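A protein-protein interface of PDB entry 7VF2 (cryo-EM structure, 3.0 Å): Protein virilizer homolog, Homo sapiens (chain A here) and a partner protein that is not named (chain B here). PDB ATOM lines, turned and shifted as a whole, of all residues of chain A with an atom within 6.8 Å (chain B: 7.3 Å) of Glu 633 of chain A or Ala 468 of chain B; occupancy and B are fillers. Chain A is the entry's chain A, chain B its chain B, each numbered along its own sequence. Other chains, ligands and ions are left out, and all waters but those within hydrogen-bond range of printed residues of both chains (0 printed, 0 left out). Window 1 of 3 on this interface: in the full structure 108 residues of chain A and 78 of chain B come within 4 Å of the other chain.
Of the 19 printed residues of chain B, 6 touch a printed residue of chain A.
Among the printed residues, no Asp or Glu carboxylate lies within 4 Å of a Lys or Arg side-chain nitrogen of the other chain.
OE2 of Glu 633 of chain A is in hydrogen-bond range of ND1 of His 636 of chain A, at 3.4 Å.
O of Leu 462 of chain B lies close to OD1 of Asn 466 of chain B (2.9 Å).
The side-chain carboxylate (OE2) of Glu 633 of chain A sits close to the backbone carbonyl oxygen (O) of Ala 464 of chain B, 3.4 Å away.
Printed residues of chain B within 4 Å of Val 562 of chain A: Ala 464 (3.5 Å).
Glu 633 of chain A touches just these residues of chain B: Ala 464, Leu 465 and Ala 468.
Printed residues of chain B within 4 Å of His 636 of chain A: Met 467 and Leu 471.
Glu 639 of chain A touches none of the printed residues of chain B.
Of the printed residues of chain A, Ala 464 of chain B touches Val 562 (3.5 Å), Glu 633 (3.4 Å) and Leu 637 (3.6 Å).
Of the printed residues of chain A, Met 467 of chain B touches His 636 and Leu 637.
Ala 468 of chain B touches just one residue of chain A: Glu 633.
The nearest residue of chain B that does not touch Glu 633 of chain A is Met 467 of chain B (4.2 Å).
The nearest printed residue of chain A that does not touch Leu 471 of chain B is Glu 633 of chain A (6.5 Å).
Ala 464 of chain B touches Val 562 of chain A (CB to CG2, 3.5 Å).
CD1 of Leu 462 of chain B touches CD2 of Leu 630 of chain A, at 3.7 Å.
Leu 630 of chain A touches Leu 465 of chain B.
Leu 465 of chain B touches Glu 633 of chain A.
Ala 468 of chain B touches Glu 633 of chain A (CB to OE1, 3.2 Å).
His 636 of chain A touches Met 467 of chain B.
CD1 of Leu 471 of chain B touches NE2 of His 636 of chain A (3.9 Å).
Ala 464 of chain B touches Leu 637 of chain A.
Leu 637 of chain A touches Met 467 of chain B (CD2 to CE, 3.7 Å).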
ATOM      1  N   PHE A 559      20.291   5.465 -20.010  1.00  0.00           N
ATOM      2  CA  PHE A 559      19.918   5.487 -18.600  1.00  0.00           C
ATOM      3  C   PHE A 559      20.562   6.665 -17.883  1.00  0.00           C
ATOM      4  O   PHE A 559      19.892   7.397 -17.141  1.00  0.00           O
ATOM      5  CB  PHE A 559      20.306   4.176 -17.924  1.00  0.00           C
ATOM      6  CG  PHE A 559      19.867   4.088 -16.499  1.00  0.00           C
ATOM      7  CD1 PHE A 559      18.559   3.791 -16.187  1.00  0.00           C
ATOM      8  CD2 PHE A 559      20.757   4.309 -15.472  1.00  0.00           C
ATOM      9  CE1 PHE A 559      18.149   3.714 -14.881  1.00  0.00           C
ATOM     10  CE2 PHE A 559      20.350   4.232 -14.164  1.00  0.00           C
ATOM     11  CZ  PHE A 559      19.045   3.935 -13.870  1.00  0.00           C
ATOM     12  N   VAL A 562      18.734   9.872 -18.941  1.00  0.00           N
ATOM     13  CA  VAL A 562      17.444  10.035 -18.272  1.00  0.00           C
ATOM     14  C   VAL A 562      17.649  10.489 -16.835  1.00  0.00           C
ATOM     15  O   VAL A 562      16.935  11.361 -16.328  1.00  0.00           O
ATOM     16  CB  VAL A 562      16.633   8.731 -18.341  1.00  0.00           C
ATOM     17  CG1 VAL A 562      15.422   8.817 -17.453  1.00  0.00           C
ATOM     18  CG2 VAL A 562      16.201   8.483 -19.756  1.00  0.00           C
ATOM     19  N   ILE A 566      16.323  13.991 -15.211  1.00  0.00           N
ATOM     20  CA  ILE A 566      15.579  14.025 -13.956  1.00  0.00           C
ATOM     21  C   ILE A 566      16.261  14.956 -12.966  1.00  0.00           C
ATOM     22  O   ILE A 566      15.603  15.737 -12.273  1.00  0.00           O
ATOM     23  CB  ILE A 566      15.424  12.608 -13.380  1.00  0.00           C
ATOM     24  CG1 ILE A 566      14.384  11.830 -14.170  1.00  0.00           C
ATOM     25  CG2 ILE A 566      15.007  12.661 -11.931  1.00  0.00           C
ATOM     26  CD1 ILE A 566      14.006  10.521 -13.540  1.00  0.00           C
ATOM     27  N   LEU A 627       8.312  14.613 -15.732  1.00  0.00           N
ATOM     28  CA  LEU A 627       9.059  14.006 -14.637  1.00  0.00           C
ATOM     29  C   LEU A 627       8.484  12.647 -14.264  1.00  0.00           C
ATOM     30  O   LEU A 627       9.228  11.717 -13.941  1.00  0.00           O
ATOM     31  CB  LEU A 627       9.055  14.941 -13.432  1.00  0.00           C
ATOM     32  CG  LEU A 627      10.028  14.631 -12.303  1.00  0.00           C
ATOM     33  CD1 LEU A 627      11.379  14.285 -12.873  1.00  0.00           C
ATOM     34  CD2 LEU A 627      10.134  15.832 -11.393  1.00  0.00           C
ATOM     35  N   ILE A 628       7.158  12.513 -14.303  1.00  0.00           N
ATOM     36  CA  ILE A 628       6.533  11.216 -14.049  1.00  0.00           C
ATOM     37  C   ILE A 628       6.949  10.213 -15.115  1.00  0.00           C
ATOM     38  O   ILE A 628       7.252   9.047 -14.822  1.00  0.00           O
ATOM     39  CB  ILE A 628       5.003  11.365 -13.988  1.00  0.00           C
ATOM     40  CG1 ILE A 628       4.575  11.914 -12.632  1.00  0.00           C
ATOM     41  CG2 ILE A 628       4.320  10.038 -14.263  1.00  0.00           C
ATOM     42  CD1 ILE A 628       3.154  12.417 -12.610  1.00  0.00           C
ATOM     43  N   ASN A 629       6.968  10.654 -16.374  1.00  0.00           N
ATOM     44  CA  ASN A 629       7.392   9.776 -17.458  1.00  0.00           C
ATOM     45  C   ASN A 629       8.852   9.374 -17.294  1.00  0.00           C
ATOM     46  O   ASN A 629       9.212   8.215 -17.519  1.00  0.00           O
ATOM     47  CB  ASN A 629       7.171  10.462 -18.804  1.00  0.00           C
ATOM     48  CG  ASN A 629       7.244   9.496 -19.965  1.00  0.00           C
ATOM     49  OD1 ASN A 629       7.317   8.284 -19.775  1.00  0.00           O
ATOM     50  ND2 ASN A 629       7.221  10.031 -21.179  1.00  0.00           N
ATOM     51  N   LEU A 630       9.700  10.311 -16.876  1.00  0.00           N
ATOM     52  CA  LEU A 630      11.109   9.991 -16.677  1.00  0.00           C
ATOM     53  C   LEU A 630      11.304   9.054 -15.492  1.00  0.00           C
ATOM     54  O   LEU A 630      12.210   8.215 -15.503  1.00  0.00           O
ATOM     55  CB  LEU A 630      11.913  11.273 -16.487  1.00  0.00           C
ATOM     56  CG  LEU A 630      12.077  12.172 -17.707  1.00  0.00           C
ATOM     57  CD1 LEU A 630      13.271  13.086 -17.533  1.00  0.00           C
ATOM     58  CD2 LEU A 630      12.229  11.334 -18.951  1.00  0.00           C
ATOM     59  N   LEU A 631      10.458   9.163 -14.469  1.00  0.00           N
ATOM     60  CA  LEU A 631      10.577   8.261 -13.327  1.00  0.00           C
ATOM     61  C   LEU A 631      10.141   6.849 -13.693  1.00  0.00           C
ATOM     62  O   LEU A 631      10.811   5.871 -13.334  1.00  0.00           O
ATOM     63  CB  LEU A 631       9.757   8.785 -12.154  1.00  0.00           C
ATOM     64  CG  LEU A 631      10.412   9.858 -11.290  1.00  0.00           C
ATOM     65  CD1 LEU A 631       9.515  10.195 -10.121  1.00  0.00           C
ATOM     66  CD2 LEU A 631      11.762   9.391 -10.805  1.00  0.00           C
ATOM     67  N   GLU A 632       9.025   6.714 -14.413  1.00  0.00           N
ATOM     68  CA  GLU A 632       8.630   5.381 -14.856  1.00  0.00           C
ATOM     69  C   GLU A 632       9.629   4.833 -15.868  1.00  0.00           C
ATOM     70  O   GLU A 632       9.816   3.616 -15.969  1.00  0.00           O
ATOM     71  CB  GLU A 632       7.213   5.388 -15.427  1.00  0.00           C
ATOM     72  CG  GLU A 632       7.022   6.208 -16.681  1.00  0.00           C
ATOM     73  CD  GLU A 632       5.573   6.254 -17.126  1.00  0.00           C
ATOM     74  OE1 GLU A 632       4.703   6.550 -16.280  1.00  0.00           O
ATOM     75  OE2 GLU A 632       5.303   5.988 -18.316  1.00  0.00           O
ATOM     76  N   GLU A 633      10.315   5.719 -16.595  1.00  0.00           N
ATOM     77  CA  GLU A 633      11.374   5.270 -17.491  1.00  0.00           C
ATOM     78  C   GLU A 633      12.575   4.753 -16.716  1.00  0.00           C
ATOM     79  O   GLU A 633      13.165   3.737 -17.091  1.00  0.00           O
ATOM     80  CB  GLU A 633      11.794   6.403 -18.422  1.00  0.00           C
ATOM     81  CG  GLU A 633      12.319   5.921 -19.750  1.00  0.00           C
ATOM     82  CD  GLU A 633      11.347   5.003 -20.447  1.00  0.00           C
ATOM     83  OE1 GLU A 633      10.131   5.286 -20.408  1.00  0.00           O
ATOM     84  OE2 GLU A 633      11.795   3.994 -21.029  1.00  0.00           O
ATOM     85  N   VAL A 634      12.968   5.447 -15.648  1.00  0.00           N
ATOM     86  CA  VAL A 634      14.042   4.947 -14.795  1.00  0.00           C
ATOM     87  C   VAL A 634      13.672   3.584 -14.228  1.00  0.00           C
ATOM     88  O   VAL A 634      14.500   2.667 -14.187  1.00  0.00           O
ATOM     89  CB  VAL A 634      14.359   5.961 -13.682  1.00  0.00           C
ATOM     90  CG1 VAL A 634      15.121   5.297 -12.562  1.00  0.00           C
ATOM     91  CG2 VAL A 634      15.161   7.111 -14.239  1.00  0.00           C
ATOM     92  N   PHE A 635      12.417   3.422 -13.806  1.00  0.00           N
ATOM     93  CA  PHE A 635      11.983   2.124 -13.297  1.00  0.00           C
ATOM     94  C   PHE A 635      12.085   1.050 -14.371  1.00  0.00           C
ATOM     95  O   PHE A 635      12.646  -0.025 -14.138  1.00  0.00           O
ATOM     96  CB  PHE A 635      10.554   2.197 -12.771  1.00  0.00           C
ATOM     97  CG  PHE A 635       9.942   0.852 -12.516  1.00  0.00           C
ATOM     98  CD1 PHE A 635      10.549  -0.047 -11.658  1.00  0.00           C
ATOM     99  CD2 PHE A 635       8.771   0.479 -13.145  1.00  0.00           C
ATOM    100  CE1 PHE A 635       9.992  -1.285 -11.426  1.00  0.00           C
ATOM    101  CE2 PHE A 635       8.212  -0.759 -12.916  1.00  0.00           C
ATOM    102  CZ  PHE A 635       8.824  -1.641 -12.055  1.00  0.00           C
ATOM    103  N   HIS A 636      11.538   1.321 -15.557  1.00  0.00           N
ATOM    104  CA  HIS A 636      11.520   0.306 -16.605  1.00  0.00           C
ATOM    105  C   HIS A 636      12.922   0.010 -17.116  1.00  0.00           C
ATOM    106  O   HIS A 636      13.183  -1.083 -17.628  1.00  0.00           O
ATOM    107  CB  HIS A 636      10.610   0.750 -17.748  1.00  0.00           C
ATOM    108  CG  HIS A 636      10.930   0.107 -19.061  1.00  0.00           C
ATOM    109  ND1 HIS A 636      11.637   0.751 -20.053  1.00  0.00           N
ATOM    110  CD2 HIS A 636      10.644  -1.125 -19.544  1.00  0.00           C
ATOM    111  CE1 HIS A 636      11.769  -0.055 -21.092  1.00  0.00           C
ATOM    112  NE2 HIS A 636      11.175  -1.200 -20.808  1.00  0.00           N
ATOM    113  N   LEU A 637      13.846   0.960 -16.971  1.00  0.00           N
ATOM    114  CA  LEU A 637      15.218   0.728 -17.406  1.00  0.00           C
ATOM    115  C   LEU A 637      15.993  -0.073 -16.374  1.00  0.00           C
ATOM    116  O   LEU A 637      16.831  -0.908 -16.730  1.00  0.00           O
ATOM    117  CB  LEU A 637      15.919   2.055 -17.674  1.00  0.00           C
ATOM    118  CG  LEU A 637      15.690   2.712 -19.029  1.00  0.00           C
ATOM    119  CD1 LEU A 637      16.463   4.003 -19.089  1.00  0.00           C
ATOM    120  CD2 LEU A 637      16.124   1.786 -20.141  1.00  0.00           C
ATOM    121  N   MET A 638      15.740   0.171 -15.090  1.00  0.00           N
ATOM    122  CA  MET A 638      16.387  -0.631 -14.060  1.00  0.00           C
ATOM    123  C   MET A 638      15.800  -2.032 -14.006  1.00  0.00           C
ATOM    124  O   MET A 638      16.467  -2.974 -13.564  1.00  0.00           O
ATOM    125  CB  MET A 638      16.264   0.060 -12.708  1.00  0.00           C
ATOM    126  CG  MET A 638      17.336   1.090 -12.458  1.00  0.00           C
ATOM    127  SD  MET A 638      17.370   1.592 -10.740  1.00  0.00           S
ATOM    128  CE  MET A 638      15.726   2.275 -10.615  1.00  0.00           C
ATOM    129  N   GLU A 639      14.556  -2.193 -14.452  1.00  0.00           N
ATOM    130  CA  GLU A 639      13.934  -3.512 -14.439  1.00  0.00           C
ATOM    131  C   GLU A 639      14.542  -4.415 -15.505  1.00  0.00           C
ATOM    132  O   GLU A 639      14.882  -5.572 -15.233  1.00  0.00           O
ATOM    133  CB  GLU A 639      12.426  -3.379 -14.632  1.00  0.00           C
ATOM    134  CG  GLU A 639      11.730  -4.674 -14.973  1.00  0.00           C
ATOM    135  CD  GLU A 639      10.227  -4.523 -15.024  1.00  0.00           C
ATOM    136  OE1 GLU A 639       9.607  -4.380 -13.951  1.00  0.00           O
ATOM    137  OE2 GLU A 639       9.666  -4.546 -16.138  1.00  0.00           O
ATOM    138  N   VAL A 707       9.852   2.811  -8.247  1.00  0.00           N
ATOM    139  CA  VAL A 707      11.310   2.768  -8.252  1.00  0.00           C
ATOM    140  C   VAL A 707      11.840   2.350  -6.886  1.00  0.00           C
ATOM    141  O   VAL A 707      12.759   1.530  -6.786  1.00  0.00           O
ATOM    142  CB  VAL A 707      11.885   4.126  -8.684  1.00  0.00           C
ATOM    143  CG1 VAL A 707      13.384   4.125  -8.535  1.00  0.00           C
ATOM    144  CG2 VAL A 707      11.499   4.433 -10.112  1.00  0.00           C
ATOM    145  N   LEU B 423      16.451   0.793 -33.522  1.00  0.00           N
ATOM    146  CA  LEU B 423      15.038   0.804 -33.160  1.00  0.00           C
ATOM    147  C   LEU B 423      14.823   0.205 -31.776  1.00  0.00           C
ATOM    148  O   LEU B 423      14.024   0.715 -30.983  1.00  0.00           O
ATOM    149  CB  LEU B 423      14.220   0.053 -34.208  1.00  0.00           C
ATOM    150  CG  LEU B 423      14.065   0.763 -35.552  1.00  0.00           C
ATOM    151  CD1 LEU B 423      13.263  -0.090 -36.513  1.00  0.00           C
ATOM    152  CD2 LEU B 423      13.411   2.114 -35.362  1.00  0.00           C
ATOM    153  N   ARG B 424      15.539  -0.875 -31.462  1.00  0.00           N
ATOM    154  CA  ARG B 424      15.401  -1.481 -30.142  1.00  0.00           C
ATOM    155  C   ARG B 424      16.061  -0.635 -29.065  1.00  0.00           C
ATOM    156  O   ARG B 424      15.730  -0.772 -27.883  1.00  0.00           O
ATOM    157  CB  ARG B 424      16.000  -2.886 -30.135  1.00  0.00           C
ATOM    158  CG  ARG B 424      15.427  -3.819 -31.180  1.00  0.00           C
ATOM    159  CD  ARG B 424      15.862  -5.252 -30.933  1.00  0.00           C
ATOM    160  NE  ARG B 424      17.191  -5.521 -31.470  1.00  0.00           N
ATOM    161  CZ  ARG B 424      18.308  -5.459 -30.754  1.00  0.00           C
ATOM    162  NH1 ARG B 424      18.258  -5.144 -29.469  1.00  0.00           N
ATOM    163  NH2 ARG B 424      19.475  -5.718 -31.322  1.00  0.00           N
ATOM    164  N   VAL B 425      16.991   0.239 -29.445  1.00  0.00           N
ATOM    165  CA  VAL B 425      17.737   1.022 -28.468  1.00  0.00           C
ATOM    166  C   VAL B 425      17.228   2.455 -28.436  1.00  0.00           C
ATOM    167  O   VAL B 425      17.007   3.022 -27.361  1.00  0.00           O
ATOM    168  CB  VAL B 425      19.241   0.994 -28.779  1.00  0.00           C
ATOM    169  CG1 VAL B 425      19.969   1.992 -27.918  1.00  0.00           C
ATOM    170  CG2 VAL B 425      19.784  -0.387 -28.564  1.00  0.00           C
ATOM    171  N   GLY B 426      17.050   3.054 -29.609  1.00  0.00           N
ATOM    172  CA  GLY B 426      16.682   4.453 -29.685  1.00  0.00           C
ATOM    173  C   GLY B 426      17.866   5.343 -29.386  1.00  0.00           C
ATOM    174  O   GLY B 426      18.744   4.965 -28.608  1.00  0.00           O
ATOM    175  N   HIS B 460      11.227  12.414 -29.391  1.00  0.00           N
ATOM    176  CA  HIS B 460      11.706  12.960 -28.132  1.00  0.00           C
ATOM    177  C   HIS B 460      13.207  13.185 -28.219  1.00  0.00           C
ATOM    178  O   HIS B 460      13.903  12.571 -29.030  1.00  0.00           O
ATOM    179  CB  HIS B 460      11.377  12.030 -26.960  1.00  0.00           C
ATOM    180  CG  HIS B 460       9.976  11.508 -26.982  1.00  0.00           C
ATOM    181  ND1 HIS B 460       8.911  12.210 -26.463  1.00  0.00           N
ATOM    182  CD2 HIS B 460       9.465  10.355 -27.472  1.00  0.00           C
ATOM    183  CE1 HIS B 460       7.804  11.507 -26.625  1.00  0.00           C
ATOM    184  NE2 HIS B 460       8.112  10.378 -27.236  1.00  0.00           N
ATOM    185  N   LEU B 462      15.256  12.629 -25.730  1.00  0.00           N
ATOM    186  CA  LEU B 462      15.906  11.629 -24.901  1.00  0.00           C
ATOM    187  C   LEU B 462      15.957  10.293 -25.626  1.00  0.00           C
ATOM    188  O   LEU B 462      15.086   9.973 -26.439  1.00  0.00           O
ATOM    189  CB  LEU B 462      15.188  11.464 -23.561  1.00  0.00           C
ATOM    190  CG  LEU B 462      15.338  12.631 -22.589  1.00  0.00           C
ATOM    191  CD1 LEU B 462      15.049  12.183 -21.172  1.00  0.00           C
ATOM    192  CD2 LEU B 462      16.725  13.228 -22.694  1.00  0.00           C
ATOM    193  N   GLY B 463      16.989   9.507 -25.321  1.00  0.00           N
ATOM    194  CA  GLY B 463      17.136   8.222 -25.979  1.00  0.00           C
ATOM    195  C   GLY B 463      16.191   7.176 -25.427  1.00  0.00           C
ATOM    196  O   GLY B 463      15.454   6.529 -26.179  1.00  0.00           O
ATOM    197  N   ALA B 464      16.206   6.985 -24.108  1.00  0.00           N
ATOM    198  CA  ALA B 464      15.305   6.016 -23.498  1.00  0.00           C
ATOM    199  C   ALA B 464      13.853   6.391 -23.740  1.00  0.00           C
ATOM    200  O   ALA B 464      12.988   5.516 -23.810  1.00  0.00           O
ATOM    201  CB  ALA B 464      15.588   5.897 -22.006  1.00  0.00           C
ATOM    202  N   LEU B 465      13.565   7.683 -23.897  1.00  0.00           N
ATOM    203  CA  LEU B 465      12.202   8.083 -24.223  1.00  0.00           C
ATOM    204  C   LEU B 465      11.832   7.674 -25.643  1.00  0.00           C
ATOM    205  O   LEU B 465      10.688   7.289 -25.900  1.00  0.00           O
ATOM    206  CB  LEU B 465      12.028   9.586 -24.030  1.00  0.00           C
ATOM    207  CG  LEU B 465      12.026  10.057 -22.578  1.00  0.00           C
ATOM    208  CD1 LEU B 465      11.438  11.450 -22.483  1.00  0.00           C
ATOM    209  CD2 LEU B 465      11.252   9.089 -21.710  1.00  0.00           C
ATOM    210  N   ASN B 466      12.784   7.729 -26.576  1.00  0.00           N
ATOM    211  CA  ASN B 466      12.514   7.224 -27.920  1.00  0.00           C
ATOM    212  C   ASN B 466      12.301   5.717 -27.905  1.00  0.00           C
ATOM    213  O   ASN B 466      11.377   5.203 -28.553  1.00  0.00           O
ATOM    214  CB  ASN B 466      13.657   7.589 -28.862  1.00  0.00           C
ATOM    215  CG  ASN B 466      13.781   9.076 -29.077  1.00  0.00           C
ATOM    216  OD1 ASN B 466      13.047   9.860 -28.484  1.00  0.00           O
ATOM    217  ND2 ASN B 466      14.713   9.475 -29.929  1.00  0.00           N
ATOM    218  N   MET B 467      13.152   4.992 -27.177  1.00  0.00           N
ATOM    219  CA  MET B 467      12.960   3.553 -27.037  1.00  0.00           C
ATOM    220  C   MET B 467      11.600   3.242 -26.428  1.00  0.00           C
ATOM    221  O   MET B 467      10.916   2.307 -26.857  1.00  0.00           O
ATOM    222  CB  MET B 467      14.073   2.949 -26.184  1.00  0.00           C
ATOM    223  CG  MET B 467      13.958   1.448 -26.016  1.00  0.00           C
ATOM    224  SD  MET B 467      15.057   0.810 -24.746  1.00  0.00           S
ATOM    225  CE  MET B 467      14.218   1.386 -23.276  1.00  0.00           C
ATOM    226  N   ALA B 468      11.187   4.026 -25.431  1.00  0.00           N
ATOM    227  CA  ALA B 468       9.906   3.787 -24.778  1.00  0.00           C
ATOM    228  C   ALA B 468       8.746   4.113 -25.703  1.00  0.00           C
ATOM    229  O   ALA B 468       7.722   3.427 -25.684  1.00  0.00           O
ATOM    230  CB  ALA B 468       9.810   4.609 -23.497  1.00  0.00           C
ATOM    231  N   ALA B 469       8.883   5.158 -26.521  1.00  0.00           N
ATOM    232  CA  ALA B 469       7.832   5.478 -27.478  1.00  0.00           C
ATOM    233  C   ALA B 469       7.673   4.366 -28.503  1.00  0.00           C
ATOM    234  O   ALA B 469       6.549   3.997 -28.861  1.00  0.00           O
ATOM    235  CB  ALA B 469       8.136   6.806 -28.168  1.00  0.00           C
ATOM    236  N   LEU B 470       8.787   3.797 -28.966  1.00  0.00           N
ATOM    237  CA  LEU B 470       8.686   2.694 -29.917  1.00  0.00           C
ATOM    238  C   LEU B 470       8.125   1.440 -29.256  1.00  0.00           C
ATOM    239  O   LEU B 470       7.304   0.727 -29.851  1.00  0.00           O
ATOM    240  CB  LEU B 470      10.046   2.409 -30.546  1.00  0.00           C
ATOM    241  CG  LEU B 470       9.936   1.885 -31.975  1.00  0.00           C
ATOM    242  CD1 LEU B 470       9.392   2.969 -32.882  1.00  0.00           C
ATOM    243  CD2 LEU B 470      11.278   1.398 -32.468  1.00  0.00           C
ATOM    244  N   LEU B 471       8.553   1.155 -28.023  1.00  0.00           N
ATOM    245  CA  LEU B 471       8.011   0.015 -27.294  1.00  0.00           C
ATOM    246  C   LEU B 471       6.519   0.183 -27.051  1.00  0.00           C
ATOM    247  O   LEU B 471       5.763  -0.790 -27.103  1.00  0.00           O
ATOM    248  CB  LEU B 471       8.750  -0.159 -25.968  1.00  0.00           C
ATOM    249  CG  LEU B 471      10.077  -0.915 -26.015  1.00  0.00           C
ATOM    250  CD1 LEU B 471      10.525  -1.292 -24.613  1.00  0.00           C
ATOM    251  CD2 LEU B 471       9.957  -2.147 -26.894  1.00  0.00           C
ATOM    252  N   ARG B 472       6.074   1.415 -26.808  1.00  0.00           N
ATOM    253  CA  ARG B 472       4.659   1.662 -26.572  1.00  0.00           C
ATOM    254  C   ARG B 472       3.860   1.520 -27.858  1.00  0.00           C
ATOM    255  O   ARG B 472       2.752   0.976 -27.854  1.00  0.00           O
ATOM    256  CB  ARG B 472       4.469   3.051 -25.970  1.00  0.00           C
ATOM    257  CG  ARG B 472       4.557   3.079 -24.463  1.00  0.00           C
ATOM    258  CD  ARG B 472       3.910   4.328 -23.918  1.00  0.00           C
ATOM    259  NE  ARG B 472       4.650   5.531 -24.286  1.00  0.00           N
ATOM    260  CZ  ARG B 472       5.629   6.058 -23.558  1.00  0.00           C
ATOM    261  NH1 ARG B 472       6.246   7.156 -23.970  1.00  0.00           N
ATOM    262  NH2 ARG B 472       5.986   5.488 -22.415  1.00  0.00           N
ATOM    263  N   LYS B 473       4.403   2.017 -28.971  1.00  0.00           N
ATOM    264  CA  LYS B 473       3.765   1.795 -30.264  1.00  0.00           C
ATOM    265  C   LYS B 473       3.583   0.308 -30.532  1.00  0.00           C
ATOM    266  O   LYS B 473       2.490  -0.145 -30.897  1.00  0.00           O
ATOM    267  CB  LYS B 473       4.591   2.438 -31.376  1.00  0.00           C
ATOM    268  CG  LYS B 473       4.265   3.892 -31.652  1.00  0.00           C
ATOM    269  CD  LYS B 473       4.943   4.357 -32.930  1.00  0.00           C
ATOM    270  CE  LYS B 473       4.674   5.827 -33.197  1.00  0.00           C
ATOM    271  NZ  LYS B 473       5.096   6.684 -32.057  1.00  0.00           N
ATOM    272  N   GLU B 474       4.644  -0.478 -30.335  1.00  0.00           N
ATOM    273  CA  GLU B 474       4.545  -1.906 -30.612  1.00  0.00           C
ATOM    274  C   GLU B 474       3.652  -2.628 -29.612  1.00  0.00           C
ATOM    275  O   GLU B 474       2.961  -3.578 -29.985  1.00  0.00           O
ATOM    276  CB  GLU B 474       5.933  -2.543 -30.636  1.00  0.00           C
ATOM    277  CG  GLU B 474       6.773  -2.109 -31.821  1.00  0.00           C
ATOM    278  CD  GLU B 474       6.187  -2.570 -33.142  1.00  0.00           C
ATOM    279  OE1 GLU B 474       5.572  -3.656 -33.177  1.00  0.00           O
ATOM    280  OE2 GLU B 474       6.333  -1.840 -34.142  1.00  0.00           O
ATOM    281  N   GLU B 506      -0.161   9.007 -26.373  1.00  0.00           N
ATOM    282  CA  GLU B 506       1.292   8.903 -26.396  1.00  0.00           C
ATOM    283  C   GLU B 506       1.855   9.729 -25.243  1.00  0.00           C
ATOM    284  O   GLU B 506       1.168  10.621 -24.731  1.00  0.00           O
ATOM    285  CB  GLU B 506       1.844   9.366 -27.742  1.00  0.00           C
ATOM    286  CG  GLU B 506       3.334   9.104 -27.926  1.00  0.00           C
ATOM    287  CD  GLU B 506       3.741   7.724 -27.435  1.00  0.00           C
ATOM    288  OE1 GLU B 506       4.438   7.640 -26.403  1.00  0.00           O
ATOM    289  OE2 GLU B 506       3.358   6.723 -28.077  1.00  0.00           O
